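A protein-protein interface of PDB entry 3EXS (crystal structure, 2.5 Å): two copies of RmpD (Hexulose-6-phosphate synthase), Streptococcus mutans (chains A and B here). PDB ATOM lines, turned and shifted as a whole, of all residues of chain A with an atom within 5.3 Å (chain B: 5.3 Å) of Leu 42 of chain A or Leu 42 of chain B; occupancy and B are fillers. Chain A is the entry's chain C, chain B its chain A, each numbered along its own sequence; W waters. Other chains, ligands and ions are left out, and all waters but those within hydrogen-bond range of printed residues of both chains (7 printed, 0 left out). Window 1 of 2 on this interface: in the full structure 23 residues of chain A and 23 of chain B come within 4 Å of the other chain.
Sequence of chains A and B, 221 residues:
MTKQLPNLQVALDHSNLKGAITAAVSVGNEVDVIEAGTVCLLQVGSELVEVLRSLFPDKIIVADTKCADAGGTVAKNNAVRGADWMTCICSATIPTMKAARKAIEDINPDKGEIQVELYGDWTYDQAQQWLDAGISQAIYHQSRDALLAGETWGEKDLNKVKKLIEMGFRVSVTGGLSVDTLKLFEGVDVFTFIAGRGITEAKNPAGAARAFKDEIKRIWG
Leu 42 of chain A touches just these residues of chain B: Leu 42, Gly 45, Ser 46, Thr 65 and Val 74. Printed residues of chain A within 4 Å of Leu 42 of chain B: Leu 42, Gly 45, Ser 46 and Thr 65. Printed residues of chain A within 4 Å of Leu 41 of chain B: Leu 41. Of the printed residues of chain B, Gln 43 of chain A touches Gly 45 (3.1 Å) and Ser 46 (2.6 Å). Of the printed residues of chain A, Val 39 of chain B touches Val 74 (3.999 Å). Of the printed residues of chain B, Gly 45 of chain A touches Leu 42 (3.5 Å), Gln 43 (3.3 Å), Val 44 (3.9 Å) and Gly 45 (3.6 Å). Printed residues of chain A within 4 Å of Gln 43 of chain B: Gly 45 and Ser 46. Asn 78 of chain B touches none of the printed residues of chain A. The nearest residue of chain B that does not touch Leu 42 of chain A is Leu 41 of chain B (4.1 Å). The nearest residue of chain A that does not touch Leu 42 of chain B is Leu 41 of chain A (4.1 Å).
The backbone carbonyl oxygen of Val 74 of chain B lies within hydrogen-bond range of the side-chain amide nitrogen of Asn 78 of chain B (2.8 Å). The side-chain amide nitrogen (ND2) of Asn 78 of chain A lies within hydrogen-bond range of the backbone carbonyl oxygen (O) of Val 74 of chain A (2.8 Å).
The backbone NH (N) of Ser 46 of chain A lies within hydrogen-bond range of the backbone carbonyl oxygen (O) of Leu 42 of chain B (3.2 Å). OG of Ser 46 of chain A sits at hydrogen-bond distance from OE1 of Gln 43 of chain B (2.6 Å). O of Leu 42 of chain A lies within hydrogen-bond range of N of Ser 46 of chain B, 3.0 Å away. The side-chain amide oxygen of Gln 43 of chain A is in hydrogen-bond range of the side-chain hydroxyl of Ser 46 of chain B (2.6 Å).
Water W4 bridges O of Gln 43 of chain B (2.5 Å) and OG of Ser 46 of chain A (3.3 Å). Water W6 lies within hydrogen-bond range of O of Val 44 of chain A (2.6 Å), O of Gln 43 of chain B (3.0 Å) and N of Ser 46 of chain A (3.0 Å). Water W3 lies within hydrogen-bond range of the side-chain amide oxygen (OE1) of Gln 43 of chain A (2.7 Å), the side-chain amide nitrogen (ND2) of Asn 78 of chain B (3.0 Å) and the backbone carbonyl oxygen (O) of Leu 42 of chain A (3.3 Å). Water W1 lies within hydrogen-bond range of the side-chain amide oxygen (OD1) of Asn 78 of chain A (2.7 Å) and the backbone carbonyl oxygen (O) of Leu 42 of chain B (2.8 Å). Water W7 bridges the backbone carbonyl oxygen of Leu 42 of chain A and the side-chain amide oxygen of Asn 78 of chain B. Water W5 lies within hydrogen-bond range of the side-chain amide oxygen of Gln 43 of chain B (2.8 Å), the side-chain amide nitrogen of Asn 78 of chain A (3.1 Å) and the backbone carbonyl oxygen of Leu 42 of chain B (3.3 Å).
Of the 13 printed residues of chain B, 9 touch a printed residue of chain A. Of the 13 printed residues of chain A, 9 touch a printed residue of chain B. Among the printed residues, no Asp or Glu carboxylate lies within 4 Å of a Lys or Arg side-chain nitrogen of the other chain.
Leu 42 of chain A touches Ser 46 of chain B, and with the chains exchanged Ser 46 of chain A touches Leu 42 of chain B. Leu 42 of chain A touches Val 74 of chain B, but with the chains exchanged Val 74 of chain A does not touch Leu 42 of chain B (4.2 Å). Gln 43 of chain A touches Gly 45 of chain B, and with the chains exchanged Gly 45 of chain A touches Gln 43 of chain B. Gly 45 of chain B touches its own counterpart, Gly 45 of chain A. Of the 18 pairs that touch across the chains among the printed residues, 17 have their exchanged pair printed and touching as well.
Among the printed residues, pairs that only touch across the chains: Gln 43 of chain A with Gly 45 of chain B, Gly 45 of chain A with Gln 43 of chain B, Leu 42 of chain A with Gly 45 of chain B, Gly 45 of chain A with Leu 42 of chain B, Leu 41 of chain A with Leu 41 of chain B, Gly 45 of chain A with Gly 45 of chain B, Val 39 of chain A with Val 74 of chain B, Leu 42 of chain A with Leu 42 of chain B, Leu 42 of chain A with Val 74 of chain B, Gly 45 of chain A with Val 44 of chain B, Val 44 of chain A with Gly 45 of chain B, Leu 42 of chain A with Thr 65 of chain B, Thr 65 of chain A with Leu 42 of chain B and Val 74 of chain A with Val 39 of chain B.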
ATOM      1  N   GLY A  37     -26.111 -13.556  32.026  1.00  0.00           N
ATOM      2  CA  GLY A  37     -27.462 -13.223  31.596  1.00  0.00           C
ATOM      3  C   GLY A  37     -27.858 -13.966  30.337  1.00  0.00           C
ATOM      4  O   GLY A  37     -26.998 -14.460  29.604  1.00  0.00           O
ATOM      5  N   THR A  38     -29.164 -14.049  30.091  1.00  0.00           N
ATOM      6  CA  THR A  38     -29.694 -14.860  29.023  1.00  0.00           C
ATOM      7  C   THR A  38     -29.265 -14.361  27.651  1.00  0.00           C
ATOM      8  O   THR A  38     -28.745 -15.149  26.829  1.00  0.00           O
ATOM      9  CB  THR A  38     -31.206 -14.917  29.107  1.00  0.00           C
ATOM     10  OG1 THR A  38     -31.558 -15.079  30.475  1.00  0.00           O
ATOM     11  CG2 THR A  38     -31.781 -16.100  28.254  1.00  0.00           C
ATOM     12  N   VAL A  39     -29.470 -13.065  27.415  1.00  0.00           N
ATOM     13  CA  VAL A  39     -28.991 -12.400  26.202  1.00  0.00           C
ATOM     14  C   VAL A  39     -27.546 -12.780  25.923  1.00  0.00           C
ATOM     15  O   VAL A  39     -27.170 -13.027  24.784  1.00  0.00           O
ATOM     16  CB  VAL A  39     -29.053 -10.883  26.355  1.00  0.00           C
ATOM     17  CG1 VAL A  39     -28.285 -10.186  25.243  1.00  0.00           C
ATOM     18  CG2 VAL A  39     -30.507 -10.414  26.413  1.00  0.00           C
ATOM     19  N   CYS A  40     -26.738 -12.835  26.975  1.00  0.00           N
ATOM     20  CA  CYS A  40     -25.356 -13.191  26.815  1.00  0.00           C
ATOM     21  C   CYS A  40     -25.106 -14.664  26.459  1.00  0.00           C
ATOM     22  O   CYS A  40     -24.345 -14.955  25.533  1.00  0.00           O
ATOM     23  CB  CYS A  40     -24.565 -12.790  28.046  1.00  0.00           C
ATOM     24  SG  CYS A  40     -22.805 -12.707  27.656  1.00  0.00           S
ATOM     25  N   LEU A  41     -25.739 -15.580  27.187  1.00  0.00           N
ATOM     26  CA  LEU A  41     -25.611 -17.029  26.920  1.00  0.00           C
ATOM     27  C   LEU A  41     -26.071 -17.418  25.503  1.00  0.00           C
ATOM     28  O   LEU A  41     -25.441 -18.251  24.843  1.00  0.00           O
ATOM     29  CB  LEU A  41     -26.374 -17.861  27.958  1.00  0.00           C
ATOM     30  CG  LEU A  41     -25.888 -17.784  29.404  1.00  0.00           C
ATOM     31  CD1 LEU A  41     -26.948 -18.355  30.354  1.00  0.00           C
ATOM     32  CD2 LEU A  41     -24.518 -18.460  29.617  1.00  0.00           C
ATOM     33  N   LEU A  42     -27.157 -16.807  25.041  1.00  0.00           N
ATOM     34  CA  LEU A  42     -27.637 -17.046  23.699  1.00  0.00           C
ATOM     35  C   LEU A  42     -26.639 -16.546  22.637  1.00  0.00           C
ATOM     36  O   LEU A  42     -26.649 -17.036  21.498  1.00  0.00           O
ATOM     37  CB  LEU A  42     -28.998 -16.397  23.500  1.00  0.00           C
ATOM     38  CG  LEU A  42     -30.164 -17.019  24.277  1.00  0.00           C
ATOM     39  CD1 LEU A  42     -31.427 -16.121  24.209  1.00  0.00           C
ATOM     40  CD2 LEU A  42     -30.480 -18.464  23.824  1.00  0.00           C
ATOM     41  N   GLN A  43     -25.766 -15.599  23.003  1.00  0.00           N
ATOM     42  CA  GLN A  43     -24.751 -15.127  22.084  1.00  0.00           C
ATOM     43  C   GLN A  43     -23.476 -15.963  22.135  1.00  0.00           C
ATOM     44  O   GLN A  43     -22.956 -16.406  21.111  1.00  0.00           O
ATOM     45  CB  GLN A  43     -24.421 -13.671  22.362  1.00  0.00           C
ATOM     46  CG  GLN A  43     -25.406 -12.694  21.798  1.00  0.00           C
ATOM     47  CD  GLN A  43     -25.363 -12.628  20.277  1.00  0.00           C
ATOM     48  OE1 GLN A  43     -25.880 -13.505  19.586  1.00  0.00           O
ATOM     49  NE2 GLN A  43     -24.768 -11.573  19.752  1.00  0.00           N
ATOM     50  N   VAL A  44     -22.963 -16.179  23.336  1.00  0.00           N
ATOM     51  CA  VAL A  44     -21.644 -16.785  23.484  1.00  0.00           C
ATOM     52  C   VAL A  44     -21.652 -18.223  23.948  1.00  0.00           C
ATOM     53  O   VAL A  44     -20.636 -18.867  23.891  1.00  0.00           O
ATOM     54  CB  VAL A  44     -20.769 -15.947  24.407  1.00  0.00           C
ATOM     55  CG1 VAL A  44     -20.957 -14.477  24.064  1.00  0.00           C
ATOM     56  CG2 VAL A  44     -21.156 -16.155  25.817  1.00  0.00           C
ATOM     57  N   GLY A  45     -22.787 -18.749  24.386  1.00  0.00           N
ATOM     58  CA  GLY A  45     -22.831 -20.132  24.823  1.00  0.00           C
ATOM     59  C   GLY A  45     -22.331 -20.319  26.251  1.00  0.00           C
ATOM     60  O   GLY A  45     -22.092 -19.350  26.971  1.00  0.00           O
ATOM     61  N   SER A  46     -22.145 -21.572  26.658  1.00  0.00           N
ATOM     62  CA  SER A  46     -21.946 -21.855  28.059  1.00  0.00           C
ATOM     63  C   SER A  46     -20.504 -21.708  28.559  1.00  0.00           C
ATOM     64  O   SER A  46     -20.259 -21.768  29.770  1.00  0.00           O
ATOM     65  CB  SER A  46     -22.549 -23.212  28.453  1.00  0.00           C
ATOM     66  OG  SER A  46     -21.778 -24.278  27.953  1.00  0.00           O
ATOM     67  N   THR A  65     -30.557 -19.193  32.288  1.00  0.00           N
ATOM     68  CA  THR A  65     -31.013 -19.838  31.052  1.00  0.00           C
ATOM     69  C   THR A  65     -32.502 -19.677  30.802  1.00  0.00           C
ATOM     70  O   THR A  65     -32.942 -19.852  29.682  1.00  0.00           O
ATOM     71  CB  THR A  65     -30.654 -21.315  30.973  1.00  0.00           C
ATOM     72  OG1 THR A  65     -31.315 -21.997  32.031  1.00  0.00           O
ATOM     73  CG2 THR A  65     -29.169 -21.530  31.087  1.00  0.00           C
ATOM     74  N   VAL A  74     -30.292 -29.011  30.144  1.00  0.00           N
ATOM     75  CA  VAL A  74     -29.833 -27.622  30.271  1.00  0.00           C
ATOM     76  C   VAL A  74     -29.144 -27.389  31.613  1.00  0.00           C
ATOM     77  O   VAL A  74     -28.028 -26.832  31.662  1.00  0.00           O
ATOM     78  CB  VAL A  74     -30.977 -26.610  30.099  1.00  0.00           C
ATOM     79  CG1 VAL A  74     -30.490 -25.213  30.448  1.00  0.00           C
ATOM     80  CG2 VAL A  74     -31.489 -26.638  28.670  1.00  0.00           C
ATOM     81  N   ASN A  78     -24.969 -26.600  32.218  1.00  0.00           N
ATOM     82  CA  ASN A  78     -24.455 -25.452  32.931  1.00  0.00           C
ATOM     83  C   ASN A  78     -23.764 -25.807  34.247  1.00  0.00           C
ATOM     84  O   ASN A  78     -22.786 -25.161  34.638  1.00  0.00           O
ATOM     85  CB  ASN A  78     -25.568 -24.429  33.099  1.00  0.00           C
ATOM     86  CG  ASN A  78     -25.914 -23.771  31.779  1.00  0.00           C
ATOM     87  OD1 ASN A  78     -25.194 -22.878  31.318  1.00  0.00           O
ATOM     88  ND2 ASN A  78     -27.005 -24.240  31.133  1.00  0.00           N
ATOM     89  N   GLY B  37     -31.870 -25.369  18.053  1.00  0.00           N
ATOM     90  CA  GLY B  37     -32.673 -25.512  19.255  1.00  0.00           C
ATOM     91  C   GLY B  37     -32.070 -24.846  20.473  1.00  0.00           C
ATOM     92  O   GLY B  37     -30.828 -24.726  20.608  1.00  0.00           O
ATOM     93  N   THR B  38     -32.959 -24.445  21.378  1.00  0.00           N
ATOM     94  CA  THR B  38     -32.578 -23.774  22.600  1.00  0.00           C
ATOM     95  C   THR B  38     -31.387 -24.428  23.296  1.00  0.00           C
ATOM     96  O   THR B  38     -30.408 -23.757  23.613  1.00  0.00           O
ATOM     97  CB  THR B  38     -33.780 -23.677  23.543  1.00  0.00           C
ATOM     98  OG1 THR B  38     -34.904 -23.205  22.791  1.00  0.00           O
ATOM     99  CG2 THR B  38     -33.509 -22.698  24.706  1.00  0.00           C
ATOM    100  N   VAL B  39     -31.468 -25.732  23.541  1.00  0.00           N
ATOM    101  CA  VAL B  39     -30.414 -26.463  24.244  1.00  0.00           C
ATOM    102  C   VAL B  39     -29.091 -26.188  23.552  1.00  0.00           C
ATOM    103  O   VAL B  39     -28.051 -25.980  24.206  1.00  0.00           O
ATOM    104  CB  VAL B  39     -30.681 -27.973  24.260  1.00  0.00           C
ATOM    105  CG1 VAL B  39     -29.469 -28.719  24.780  1.00  0.00           C
ATOM    106  CG2 VAL B  39     -31.933 -28.299  25.060  1.00  0.00           C
ATOM    107  N   CYS B  40     -29.144 -26.136  22.225  1.00  0.00           N
ATOM    108  CA  CYS B  40     -27.933 -25.968  21.467  1.00  0.00           C
ATOM    109  C   CYS B  40     -27.408 -24.538  21.546  1.00  0.00           C
ATOM    110  O   CYS B  40     -26.217 -24.349  21.760  1.00  0.00           O
ATOM    111  CB  CYS B  40     -28.103 -26.445  20.014  1.00  0.00           C
ATOM    112  SG  CYS B  40     -26.484 -26.754  19.202  1.00  0.00           S
ATOM    113  N   LEU B  41     -28.286 -23.548  21.394  1.00  0.00           N
ATOM    114  CA  LEU B  41     -27.893 -22.141  21.426  1.00  0.00           C
ATOM    115  C   LEU B  41     -27.303 -21.748  22.773  1.00  0.00           C
ATOM    116  O   LEU B  41     -26.289 -21.041  22.840  1.00  0.00           O
ATOM    117  CB  LEU B  41     -29.080 -21.231  21.115  1.00  0.00           C
ATOM    118  CG  LEU B  41     -29.684 -21.235  19.700  1.00  0.00           C
ATOM    119  CD1 LEU B  41     -30.993 -20.508  19.685  1.00  0.00           C
ATOM    120  CD2 LEU B  41     -28.722 -20.656  18.654  1.00  0.00           C
ATOM    121  N   LEU B  42     -27.928 -22.226  23.842  1.00  0.00           N
ATOM    122  CA  LEU B  42     -27.424 -22.021  25.182  1.00  0.00           C
ATOM    123  C   LEU B  42     -26.031 -22.632  25.356  1.00  0.00           C
ATOM    124  O   LEU B  42     -25.285 -22.198  26.229  1.00  0.00           O
ATOM    125  CB  LEU B  42     -28.415 -22.559  26.226  1.00  0.00           C
ATOM    126  CG  LEU B  42     -29.742 -21.778  26.376  1.00  0.00           C
ATOM    127  CD1 LEU B  42     -30.736 -22.565  27.201  1.00  0.00           C
ATOM    128  CD2 LEU B  42     -29.536 -20.369  27.003  1.00  0.00           C
ATOM    129  N   GLN B  43     -25.666 -23.609  24.519  1.00  0.00           N
ATOM    130  CA  GLN B  43     -24.320 -24.202  24.582  1.00  0.00           C
ATOM    131  C   GLN B  43     -23.263 -23.522  23.731  1.00  0.00           C
ATOM    132  O   GLN B  43     -22.135 -23.294  24.168  1.00  0.00           O
ATOM    133  CB  GLN B  43     -24.359 -25.686  24.223  1.00  0.00           C
ATOM    134  CG  GLN B  43     -24.806 -26.571  25.394  1.00  0.00           C
ATOM    135  CD  GLN B  43     -23.774 -26.670  26.502  1.00  0.00           C
ATOM    136  OE1 GLN B  43     -23.751 -25.855  27.420  1.00  0.00           O
ATOM    137  NE2 GLN B  43     -22.947 -27.688  26.439  1.00  0.00           N
ATOM    138  N   VAL B  44     -23.633 -23.214  22.498  1.00  0.00           N
ATOM    139  CA  VAL B  44     -22.652 -22.816  21.489  1.00  0.00           C
ATOM    140  C   VAL B  44     -22.793 -21.344  21.115  1.00  0.00           C
ATOM    141  O   VAL B  44     -21.875 -20.777  20.539  1.00  0.00           O
ATOM    142  CB  VAL B  44     -22.690 -23.766  20.241  1.00  0.00           C
ATOM    143  CG1 VAL B  44     -22.411 -25.217  20.665  1.00  0.00           C
ATOM    144  CG2 VAL B  44     -23.990 -23.695  19.541  1.00  0.00           C
ATOM    145  N   GLY B  45     -23.912 -20.719  21.477  1.00  0.00           N
ATOM    146  CA  GLY B  45     -24.157 -19.316  21.144  1.00  0.00           C
ATOM    147  C   GLY B  45     -24.689 -19.156  19.724  1.00  0.00           C
ATOM    148  O   GLY B  45     -24.930 -20.143  19.026  1.00  0.00           O
ATOM    149  N   SER B  46     -24.863 -17.929  19.272  1.00  0.00           N
ATOM    150  CA  SER B  46     -25.555 -17.726  18.016  1.00  0.00           C
ATOM    151  C   SER B  46     -24.713 -17.899  16.748  1.00  0.00           C
ATOM    152  O   SER B  46     -25.249 -17.782  15.638  1.00  0.00           O
ATOM    153  CB  SER B  46     -26.170 -16.348  17.988  1.00  0.00           C
ATOM    154  OG  SER B  46     -25.135 -15.398  17.951  1.00  0.00           O
ATOM    155  N   THR B  65     -34.890 -19.360  20.571  1.00  0.00           N
ATOM    156  CA  THR B  65     -34.339 -18.693  21.731  1.00  0.00           C
ATOM    157  C   THR B  65     -35.316 -18.679  22.890  1.00  0.00           C
ATOM    158  O   THR B  65     -34.904 -18.526  24.035  1.00  0.00           O
ATOM    159  CB  THR B  65     -33.950 -17.269  21.414  1.00  0.00           C
ATOM    160  OG1 THR B  65     -35.106 -16.589  20.915  1.00  0.00           O
ATOM    161  CG2 THR B  65     -32.826 -17.230  20.389  1.00  0.00           C
ATOM    162  N   VAL B  74     -32.285  -9.646  21.562  1.00  0.00           N
ATOM    163  CA  VAL B  74     -32.227 -11.056  21.177  1.00  0.00           C
ATOM    164  C   VAL B  74     -32.665 -11.316  19.727  1.00  0.00           C
ATOM    165  O   VAL B  74     -32.053 -12.137  19.031  1.00  0.00           O
ATOM    166  CB  VAL B  74     -33.022 -11.967  22.131  1.00  0.00           C
ATOM    167  CG1 VAL B  74     -32.750 -13.413  21.785  1.00  0.00           C
ATOM    168  CG2 VAL B  74     -32.656 -11.681  23.583  1.00  0.00           C
ATOM    169  N   ASN B  78     -29.897 -12.473  16.643  1.00  0.00           N
ATOM    170  CA  ASN B  78     -30.052 -13.682  15.834  1.00  0.00           C
ATOM    171  C   ASN B  78     -30.339 -13.379  14.361  1.00  0.00           C
ATOM    172  O   ASN B  78     -29.945 -14.135  13.482  1.00  0.00           O
ATOM    173  CB  ASN B  78     -31.089 -14.621  16.445  1.00  0.00           C
ATOM    174  CG  ASN B  78     -30.580 -15.267  17.708  1.00  0.00           C
ATOM    175  OD1 ASN B  78     -30.006 -16.365  17.659  1.00  0.00           O
ATOM    176  ND2 ASN B  78     -30.716 -14.563  18.851  1.00  0.00           N
HETATM  177  O   HOH W   1     -25.970 -22.011  28.910  1.00  0.00           O
HETATM  178  O   HOH W   2     -21.603 -18.325  19.176  1.00  0.00           O
HETATM  179  O   HOH W   3     -28.233 -14.352  20.532  1.00  0.00           O
HETATM  180  O   HOH W   4     -20.775 -25.164  24.989  1.00  0.00           O
HETATM  181  O   HOH W   5     -26.189 -24.649  28.206  1.00  0.00           O
HETATM  182  O   HOH W   6     -19.956 -21.320  24.626  1.00  0.00           O
HETATM  183  O   HOH W   7     -28.968 -17.330  20.119  1.00  0.00           O
